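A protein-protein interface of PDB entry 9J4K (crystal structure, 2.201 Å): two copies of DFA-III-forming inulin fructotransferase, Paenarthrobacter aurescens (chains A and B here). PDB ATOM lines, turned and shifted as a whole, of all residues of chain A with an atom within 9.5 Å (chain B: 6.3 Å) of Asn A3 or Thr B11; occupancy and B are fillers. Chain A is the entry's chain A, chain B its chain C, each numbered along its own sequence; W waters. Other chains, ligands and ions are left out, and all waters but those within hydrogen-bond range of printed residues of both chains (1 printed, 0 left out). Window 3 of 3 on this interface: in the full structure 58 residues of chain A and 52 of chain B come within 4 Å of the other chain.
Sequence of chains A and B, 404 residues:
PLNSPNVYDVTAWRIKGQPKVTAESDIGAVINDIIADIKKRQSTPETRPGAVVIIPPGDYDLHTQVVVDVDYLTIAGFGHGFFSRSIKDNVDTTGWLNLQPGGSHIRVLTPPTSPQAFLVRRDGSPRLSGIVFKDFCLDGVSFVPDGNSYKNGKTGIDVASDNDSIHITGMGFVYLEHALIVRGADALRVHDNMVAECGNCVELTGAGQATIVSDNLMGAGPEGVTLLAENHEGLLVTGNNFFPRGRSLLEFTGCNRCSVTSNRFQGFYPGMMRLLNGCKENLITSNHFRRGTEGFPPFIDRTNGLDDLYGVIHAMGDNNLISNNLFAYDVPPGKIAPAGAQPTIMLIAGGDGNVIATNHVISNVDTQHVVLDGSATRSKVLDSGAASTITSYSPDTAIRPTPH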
ATOM      1  N   PRO A   1      19.247  33.761 -14.143  1.00  0.00           N
ATOM      2  CA  PRO A   1      18.240  34.434 -14.989  1.00  0.00           C
ATOM      3  C   PRO A   1      17.562  33.467 -15.980  1.00  0.00           C
ATOM      4  O   PRO A   1      16.353  33.325 -15.931  1.00  0.00           O
ATOM      5  CB  PRO A   1      19.013  35.546 -15.722  1.00  0.00           C
ATOM      6  CG  PRO A   1      20.470  35.111 -15.677  1.00  0.00           C
ATOM      7  CD  PRO A   1      20.605  34.245 -14.441  1.00  0.00           C
ATOM      8  N   LEU A   2      18.347  32.843 -16.863  1.00  0.00           N
ATOM      9  CA  LEU A   2      17.939  31.691 -17.714  1.00  0.00           C
ATOM     10  C   LEU A   2      18.708  30.460 -17.220  1.00  0.00           C
ATOM     11  O   LEU A   2      19.691  30.653 -16.472  1.00  0.00           O
ATOM     12  CB  LEU A   2      18.239  32.027 -19.178  1.00  0.00           C
ATOM     13  CG  LEU A   2      17.379  33.151 -19.768  1.00  0.00           C
ATOM     14  CD1 LEU A   2      17.928  33.637 -21.097  1.00  0.00           C
ATOM     15  CD2 LEU A   2      15.939  32.698 -19.946  1.00  0.00           C
ATOM     16  N   ASN A   3      18.280  29.245 -17.576  1.00  0.00           N
ATOM     17  CA  ASN A   3      18.873  27.996 -17.020  1.00  0.00           C
ATOM     18  C   ASN A   3      20.124  27.612 -17.819  1.00  0.00           C
ATOM     19  O   ASN A   3      20.313  26.415 -18.088  1.00  0.00           O
ATOM     20  CB  ASN A   3      17.868  26.840 -16.971  1.00  0.00           C
ATOM     21  CG  ASN A   3      18.291  25.756 -16.001  1.00  0.00           C
ATOM     22  OD1 ASN A   3      18.761  26.052 -14.905  1.00  0.00           O
ATOM     23  ND2 ASN A   3      18.133  24.501 -16.390  1.00  0.00           N
ATOM     24  N   SER A   4      20.924  28.606 -18.212  1.00  0.00           N
ATOM     25  CA  SER A   4      22.175  28.438 -18.986  1.00  0.00           C
ATOM     26  C   SER A   4      23.285  29.195 -18.281  1.00  0.00           C
ATOM     27  O   SER A   4      23.091  30.349 -17.899  1.00  0.00           O
ATOM     28  CB  SER A   4      22.023  28.928 -20.389  1.00  0.00           C
ATOM     29  OG  SER A   4      23.286  29.004 -21.023  1.00  0.00           O
ATOM     30  N   PRO A   5      24.490  28.596 -18.153  1.00  0.00           N
ATOM     31  CA  PRO A   5      25.626  29.298 -17.566  1.00  0.00           C
ATOM     32  C   PRO A   5      26.235  30.297 -18.561  1.00  0.00           C
ATOM     33  O   PRO A   5      27.141  30.995 -18.173  1.00  0.00           O
ATOM     34  CB  PRO A   5      26.597  28.155 -17.237  1.00  0.00           C
ATOM     35  CG  PRO A   5      26.314  27.110 -18.307  1.00  0.00           C
ATOM     36  CD  PRO A   5      24.830  27.229 -18.591  1.00  0.00           C
ATOM     37  N   ASN A   6      25.726  30.329 -19.801  1.00  0.00           N
ATOM     38  CA  ASN A   6      26.225  31.192 -20.909  1.00  0.00           C
ATOM     39  C   ASN A   6      25.418  32.495 -20.962  1.00  0.00           C
ATOM     40  O   ASN A   6      25.589  33.254 -21.942  1.00  0.00           O
ATOM     41  CB  ASN A   6      26.190  30.439 -22.238  1.00  0.00           C
ATOM     42  CG  ASN A   6      27.012  29.167 -22.184  1.00  0.00           C
ATOM     43  OD1 ASN A   6      28.030  29.110 -21.497  1.00  0.00           O
ATOM     44  ND2 ASN A   6      26.589  28.149 -22.912  1.00  0.00           N
ATOM     45  N   VAL A   7      24.571  32.747 -19.959  1.00  0.00           N
ATOM     46  CA  VAL A   7      23.777  34.006 -19.846  1.00  0.00           C
ATOM     47  C   VAL A   7      24.187  34.707 -18.551  1.00  0.00           C
ATOM     48  O   VAL A   7      23.984  34.132 -17.481  1.00  0.00           O
ATOM     49  CB  VAL A   7      22.259  33.759 -19.902  1.00  0.00           C
ATOM     50  CG1 VAL A   7      21.468  35.035 -19.645  1.00  0.00           C
ATOM     51  CG2 VAL A   7      21.858  33.146 -21.228  1.00  0.00           C
ATOM     52  N   TYR A   8      24.737  35.916 -18.671  1.00  0.00           N
ATOM     53  CA  TYR A   8      25.285  36.702 -17.541  1.00  0.00           C
ATOM     54  C   TYR A   8      24.587  38.055 -17.468  1.00  0.00           C
ATOM     55  O   TYR A   8      24.481  38.752 -18.491  1.00  0.00           O
ATOM     56  CB  TYR A   8      26.782  36.956 -17.713  1.00  0.00           C
ATOM     57  CG  TYR A   8      27.651  35.726 -17.715  1.00  0.00           C
ATOM     58  CD1 TYR A   8      27.961  35.081 -18.899  1.00  0.00           C
ATOM     59  CD2 TYR A   8      28.211  35.245 -16.540  1.00  0.00           C
ATOM     60  CE1 TYR A   8      28.789  33.972 -18.918  1.00  0.00           C
ATOM     61  CE2 TYR A   8      29.040  34.132 -16.542  1.00  0.00           C
ATOM     62  CZ  TYR A   8      29.332  33.499 -17.737  1.00  0.00           C
ATOM     63  OH  TYR A   8      30.140  32.404 -17.758  1.00  0.00           O
ATOM     64  N   ASP B   9      12.117  29.200 -21.923  1.00  0.00           N
ATOM     65  CA  ASP B   9      13.591  29.057 -22.000  1.00  0.00           C
ATOM     66  C   ASP B   9      13.863  27.593 -22.357  1.00  0.00           C
ATOM     67  O   ASP B   9      13.488  26.733 -21.539  1.00  0.00           O
ATOM     68  CB  ASP B   9      14.215  29.522 -20.687  1.00  0.00           C
ATOM     69  CG  ASP B   9      15.671  29.122 -20.517  1.00  0.00           C
ATOM     70  OD1 ASP B   9      16.242  28.554 -21.469  1.00  0.00           O
ATOM     71  OD2 ASP B   9      16.209  29.367 -19.426  1.00  0.00           O
ATOM     72  N   VAL B  10      14.453  27.308 -23.528  1.00  0.00           N
ATOM     73  CA  VAL B  10      14.641  25.899 -24.011  1.00  0.00           C
ATOM     74  C   VAL B  10      15.477  25.119 -22.995  1.00  0.00           C
ATOM     75  O   VAL B  10      15.330  23.895 -22.969  1.00  0.00           O
ATOM     76  CB  VAL B  10      15.260  25.772 -25.421  1.00  0.00           C
ATOM     77  CG1 VAL B  10      14.319  26.263 -26.505  1.00  0.00           C
ATOM     78  CG2 VAL B  10      16.626  26.430 -25.544  1.00  0.00           C
ATOM     79  N   THR B  11      16.319  25.792 -22.200  1.00  0.00           N
ATOM     80  CA  THR B  11      17.251  25.136 -21.244  1.00  0.00           C
ATOM     81  C   THR B  11      16.532  24.842 -19.924  1.00  0.00           C
ATOM     82  O   THR B  11      17.030  23.992 -19.178  1.00  0.00           O
ATOM     83  CB  THR B  11      18.539  25.951 -21.043  1.00  0.00           C
ATOM     84  OG1 THR B  11      18.233  27.185 -20.392  1.00  0.00           O
ATOM     85  CG2 THR B  11      19.262  26.208 -22.349  1.00  0.00           C
ATOM     86  N   ALA B  12      15.405  25.503 -19.653  1.00  0.00           N
ATOM     87  CA  ALA B  12      14.600  25.309 -18.423  1.00  0.00           C
ATOM     88  C   ALA B  12      13.473  24.302 -18.670  1.00  0.00           C
ATOM     89  O   ALA B  12      13.007  23.707 -17.686  1.00  0.00           O
ATOM     90  CB  ALA B  12      14.032  26.624 -17.941  1.00  0.00           C
ATOM     91  N   TRP B  13      13.014  24.148 -19.913  1.00  0.00           N
ATOM     92  CA  TRP B  13      11.820  23.322 -20.235  1.00  0.00           C
ATOM     93  C   TRP B  13      12.168  21.841 -20.087  1.00  0.00           C
ATOM     94  O   TRP B  13      13.193  21.403 -20.631  1.00  0.00           O
ATOM     95  CB  TRP B  13      11.267  23.627 -21.631  1.00  0.00           C
ATOM     96  CG  TRP B  13       9.970  22.927 -21.898  1.00  0.00           C
ATOM     97  CD1 TRP B  13       9.795  21.759 -22.581  1.00  0.00           C
ATOM     98  CD2 TRP B  13       8.662  23.333 -21.455  1.00  0.00           C
ATOM     99  NE1 TRP B  13       8.473  21.421 -22.607  1.00  0.00           N
ATOM    100  CE2 TRP B  13       7.750  22.365 -21.929  1.00  0.00           C
ATOM    101  CE3 TRP B  13       8.172  24.420 -20.721  1.00  0.00           C
ATOM    102  CZ2 TRP B  13       6.382  22.446 -21.678  1.00  0.00           C
ATOM    103  CZ3 TRP B  13       6.821  24.492 -20.463  1.00  0.00           C
ATOM    104  CH2 TRP B  13       5.942  23.516 -20.935  1.00  0.00           C
ATOM    105  N   ARG B  14      11.336  21.108 -19.357  1.00  0.00           N
ATOM    106  CA  ARG B  14      11.464  19.641 -19.182  1.00  0.00           C
ATOM    107  C   ARG B  14      10.224  19.000 -19.796  1.00  0.00           C
ATOM    108  O   ARG B  14       9.121  19.490 -19.525  1.00  0.00           O
ATOM    109  CB  ARG B  14      11.652  19.296 -17.702  1.00  0.00           C
ATOM    110  CG  ARG B  14      13.078  19.493 -17.203  1.00  0.00           C
ATOM    111  CD  ARG B  14      14.060  18.503 -17.824  1.00  0.00           C
ATOM    112  NE  ARG B  14      15.447  18.898 -17.620  1.00  0.00           N
ATOM    113  CZ  ARG B  14      16.078  19.870 -18.281  1.00  0.00           C
ATOM    114  NH1 ARG B  14      15.453  20.570 -19.214  1.00  0.00           N
ATOM    115  NH2 ARG B  14      17.341  20.141 -17.995  1.00  0.00           N
ATOM    116  N   ALA B  23      17.509  20.467 -24.338  1.00  0.00           N
ATOM    117  CA  ALA B  23      17.901  21.348 -25.456  1.00  0.00           C
ATOM    118  C   ALA B  23      19.190  20.794 -26.074  1.00  0.00           C
ATOM    119  O   ALA B  23      19.308  20.807 -27.306  1.00  0.00           O
ATOM    120  CB  ALA B  23      18.056  22.764 -24.961  1.00  0.00           C
ATOM    121  N   GLU B  24      20.108  20.300 -25.235  1.00  0.00           N
ATOM    122  CA  GLU B  24      21.431  19.790 -25.675  1.00  0.00           C
ATOM    123  C   GLU B  24      21.228  18.507 -26.480  1.00  0.00           C
ATOM    124  O   GLU B  24      21.839  18.406 -27.553  1.00  0.00           O
ATOM    125  CB  GLU B  24      22.367  19.542 -24.487  1.00  0.00           C
ATOM    126  CG  GLU B  24      22.837  20.811 -23.793  1.00  0.00           C
ATOM    127  CD  GLU B  24      21.853  21.482 -22.842  1.00  0.00           C
ATOM    128  OE1 GLU B  24      20.824  20.855 -22.479  1.00  0.00           O
ATOM    129  OE2 GLU B  24      22.114  22.647 -22.469  1.00  0.00           O
ATOM    130  N   VAL B  30      12.285  19.259 -27.660  1.00  0.00           N
ATOM    131  CA  VAL B  30      11.951  20.260 -26.601  1.00  0.00           C
ATOM    132  C   VAL B  30      10.988  21.295 -27.196  1.00  0.00           C
ATOM    133  O   VAL B  30       9.964  21.565 -26.571  1.00  0.00           O
ATOM    134  CB  VAL B  30      13.219  20.921 -26.024  1.00  0.00           C
ATOM    135  CG1 VAL B  30      12.888  22.029 -25.041  1.00  0.00           C
ATOM    136  CG2 VAL B  30      14.146  19.895 -25.382  1.00  0.00           C
ATOM    137  N   ILE B  54      13.155  31.067 -26.168  1.00  0.00           N
ATOM    138  CA  ILE B  54      14.476  31.713 -25.925  1.00  0.00           C
ATOM    139  C   ILE B  54      15.547  30.623 -25.966  1.00  0.00           C
ATOM    140  O   ILE B  54      15.413  29.628 -25.239  1.00  0.00           O
ATOM    141  CB  ILE B  54      14.492  32.489 -24.595  1.00  0.00           C
ATOM    142  CG1 ILE B  54      13.385  33.545 -24.511  1.00  0.00           C
ATOM    143  CG2 ILE B  54      15.869  33.099 -24.352  1.00  0.00           C
ATOM    144  CD1 ILE B  54      13.485  34.629 -25.563  1.00  0.00           C
ATOM    145  N   ILE B  55      16.570  30.816 -26.792  1.00  0.00           N
ATOM    146  CA  ILE B  55      17.713  29.875 -26.950  1.00  0.00           C
ATOM    147  C   ILE B  55      18.965  30.579 -26.450  1.00  0.00           C
ATOM    148  O   ILE B  55      19.590  31.330 -27.201  1.00  0.00           O
ATOM    149  CB  ILE B  55      17.864  29.426 -28.412  1.00  0.00           C
ATOM    150  CG1 ILE B  55      16.518  29.008 -29.014  1.00  0.00           C
ATOM    151  CG2 ILE B  55      18.926  28.336 -28.512  1.00  0.00           C
ATOM    152  CD1 ILE B  55      16.602  28.501 -30.438  1.00  0.00           C
ATOM    153  N   PRO B  56      19.360  30.356 -25.176  1.00  0.00           N
ATOM    154  CA  PRO B  56      20.618  30.891 -24.654  1.00  0.00           C
ATOM    155  C   PRO B  56      21.773  30.465 -25.542  1.00  0.00           C
ATOM    156  O   PRO B  56      21.666  29.468 -26.258  1.00  0.00           O
ATOM    157  CB  PRO B  56      20.752  30.247 -23.259  1.00  0.00           C
ATOM    158  CG  PRO B  56      19.323  29.934 -22.871  1.00  0.00           C
ATOM    159  CD  PRO B  56      18.631  29.571 -24.171  1.00  0.00           C
ATOM    160  N   PRO B  57      22.925  31.164 -25.492  1.00  0.00           N
ATOM    161  CA  PRO B  57      24.123  30.680 -26.177  1.00  0.00           C
ATOM    162  C   PRO B  57      24.472  29.276 -25.652  1.00  0.00           C
ATOM    163  O   PRO B  57      24.273  29.021 -24.476  1.00  0.00           O
ATOM    164  CB  PRO B  57      25.182  31.743 -25.838  1.00  0.00           C
ATOM    165  CG  PRO B  57      24.358  32.975 -25.502  1.00  0.00           C
ATOM    166  CD  PRO B  57      23.156  32.421 -24.768  1.00  0.00           C
ATOM    167  N   TYR B  60      23.558  22.875 -29.194  1.00  0.00           N
ATOM    168  CA  TYR B  60      22.294  22.112 -29.098  1.00  0.00           C
ATOM    169  C   TYR B  60      22.180  21.245 -30.352  1.00  0.00           C
ATOM    170  O   TYR B  60      22.320  21.772 -31.461  1.00  0.00           O
ATOM    171  CB  TYR B  60      21.110  23.066 -28.932  1.00  0.00           C
ATOM    172  CG  TYR B  60      21.276  24.133 -27.875  1.00  0.00           C
ATOM    173  CD1 TYR B  60      21.076  23.853 -26.536  1.00  0.00           C
ATOM    174  CD2 TYR B  60      21.561  25.444 -28.219  1.00  0.00           C
ATOM    175  CE1 TYR B  60      21.199  24.832 -25.560  1.00  0.00           C
ATOM    176  CE2 TYR B  60      21.681  26.440 -27.260  1.00  0.00           C
ATOM    177  CZ  TYR B  60      21.495  26.135 -25.924  1.00  0.00           C
ATOM    178  OH  TYR B  60      21.633  27.097 -24.963  1.00  0.00           O
HETATM  179  O   HOH W   1      23.197  27.050 -22.614  1.00  0.00           O
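OD2 of Asp B9 sits at hydrogen-bond distance from N of Asn A3 (2.8 Å).
O of Thr B11 lies within hydrogen-bond range of ND2 of Asn A3 (3.0 Å).
The side-chain amide nitrogen (ND2) of Asn A6 sits at hydrogen-bond distance from the backbone carbonyl oxygen (O) of Pro B57, 2.9 Å away.
The side-chain hydroxyl (OG) of Ser A4 is in hydrogen-bond range of the backbone NH (N) of Asn A6, at 3.0 Å.
The side-chain hydroxyl of Thr B11 is in hydrogen-bond range of the side-chain carboxylate of Asp B9 (2.6 Å).
O of Ile B54 is in hydrogen-bond range of N of Val B10, 3.0 Å away.
The side-chain hydroxyl of Tyr B60 lies within hydrogen-bond range of the backbone carbonyl oxygen of Pro B56 (2.7 Å).
O of Pro B57 lies within hydrogen-bond range of OH of Tyr B60 (3.3 Å).
Among the printed residues, pairs that only touch across the chains: Leu A2 with Asp B9, Ser A4 with Pro B56, Ser A4 with Pro B57, Val A7 with Pro B56, Ser A4 with Thr B11, Val A7 with Pro B57, Asn A3 with Ala B12 and Leu A2 with Ile B54.
Of the printed residues of chain B, Leu A2 touches Asp B9 and Ile B54.
Asn A3 touches just these residues of chain B: Asp B9 (2.8 Å), Thr B11 (3.0 Å) and Ala B12 (3.9 Å).
Tyr A8 touches none of the printed residues of chain B.
Asp B9 touches two residues of chain A.
No residue of chain A comes within 4 Å of Val B10.
Of the printed residues of chain A, Thr B11 touches Asn A3 and Ser A4.
Printed residues of chain A within 4 Å of Ala B12: Asn A3 (3.9 Å).
Trp B13 touches none of the printed residues of chain A.
Printed residues of chain A within 4 Å of Pro B57: Ser A4, Asn A6 and Val A7.
The nearest printed residue of chain B that does not touch Asn A6 is Tyr B60 (5.5 Å).
Of the 14 printed residues of chain B, 6 touch a printed residue of chain A.
Hydrophobic or aromatic side chains of chain B that line the printed part of chain A: Ala B12, Ile B54, Pro B56 and Pro B57.
Of the 8 printed residues of chain A, 5 touch a printed residue of chain B.
Printed residues of chain A that touch a printed residue of chain B: Leu A2, Asn A3, Ser A4, Asn A6 and Val A7.
Among the printed residues, 11 pairs touch across the chains.
Among the printed residues, no Asp or Glu carboxylate lies within 4 Å of a Lys or Arg side-chain nitrogen of the other chain.
No position is printed for both chains.
Of the 11 pairs that touch across the chains among the printed residues, none has its exchanged pair printed and touching as well.
Water W1 lies within hydrogen-bond range of OG of Ser A4, OH of Tyr B60 and O of Pro B57.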
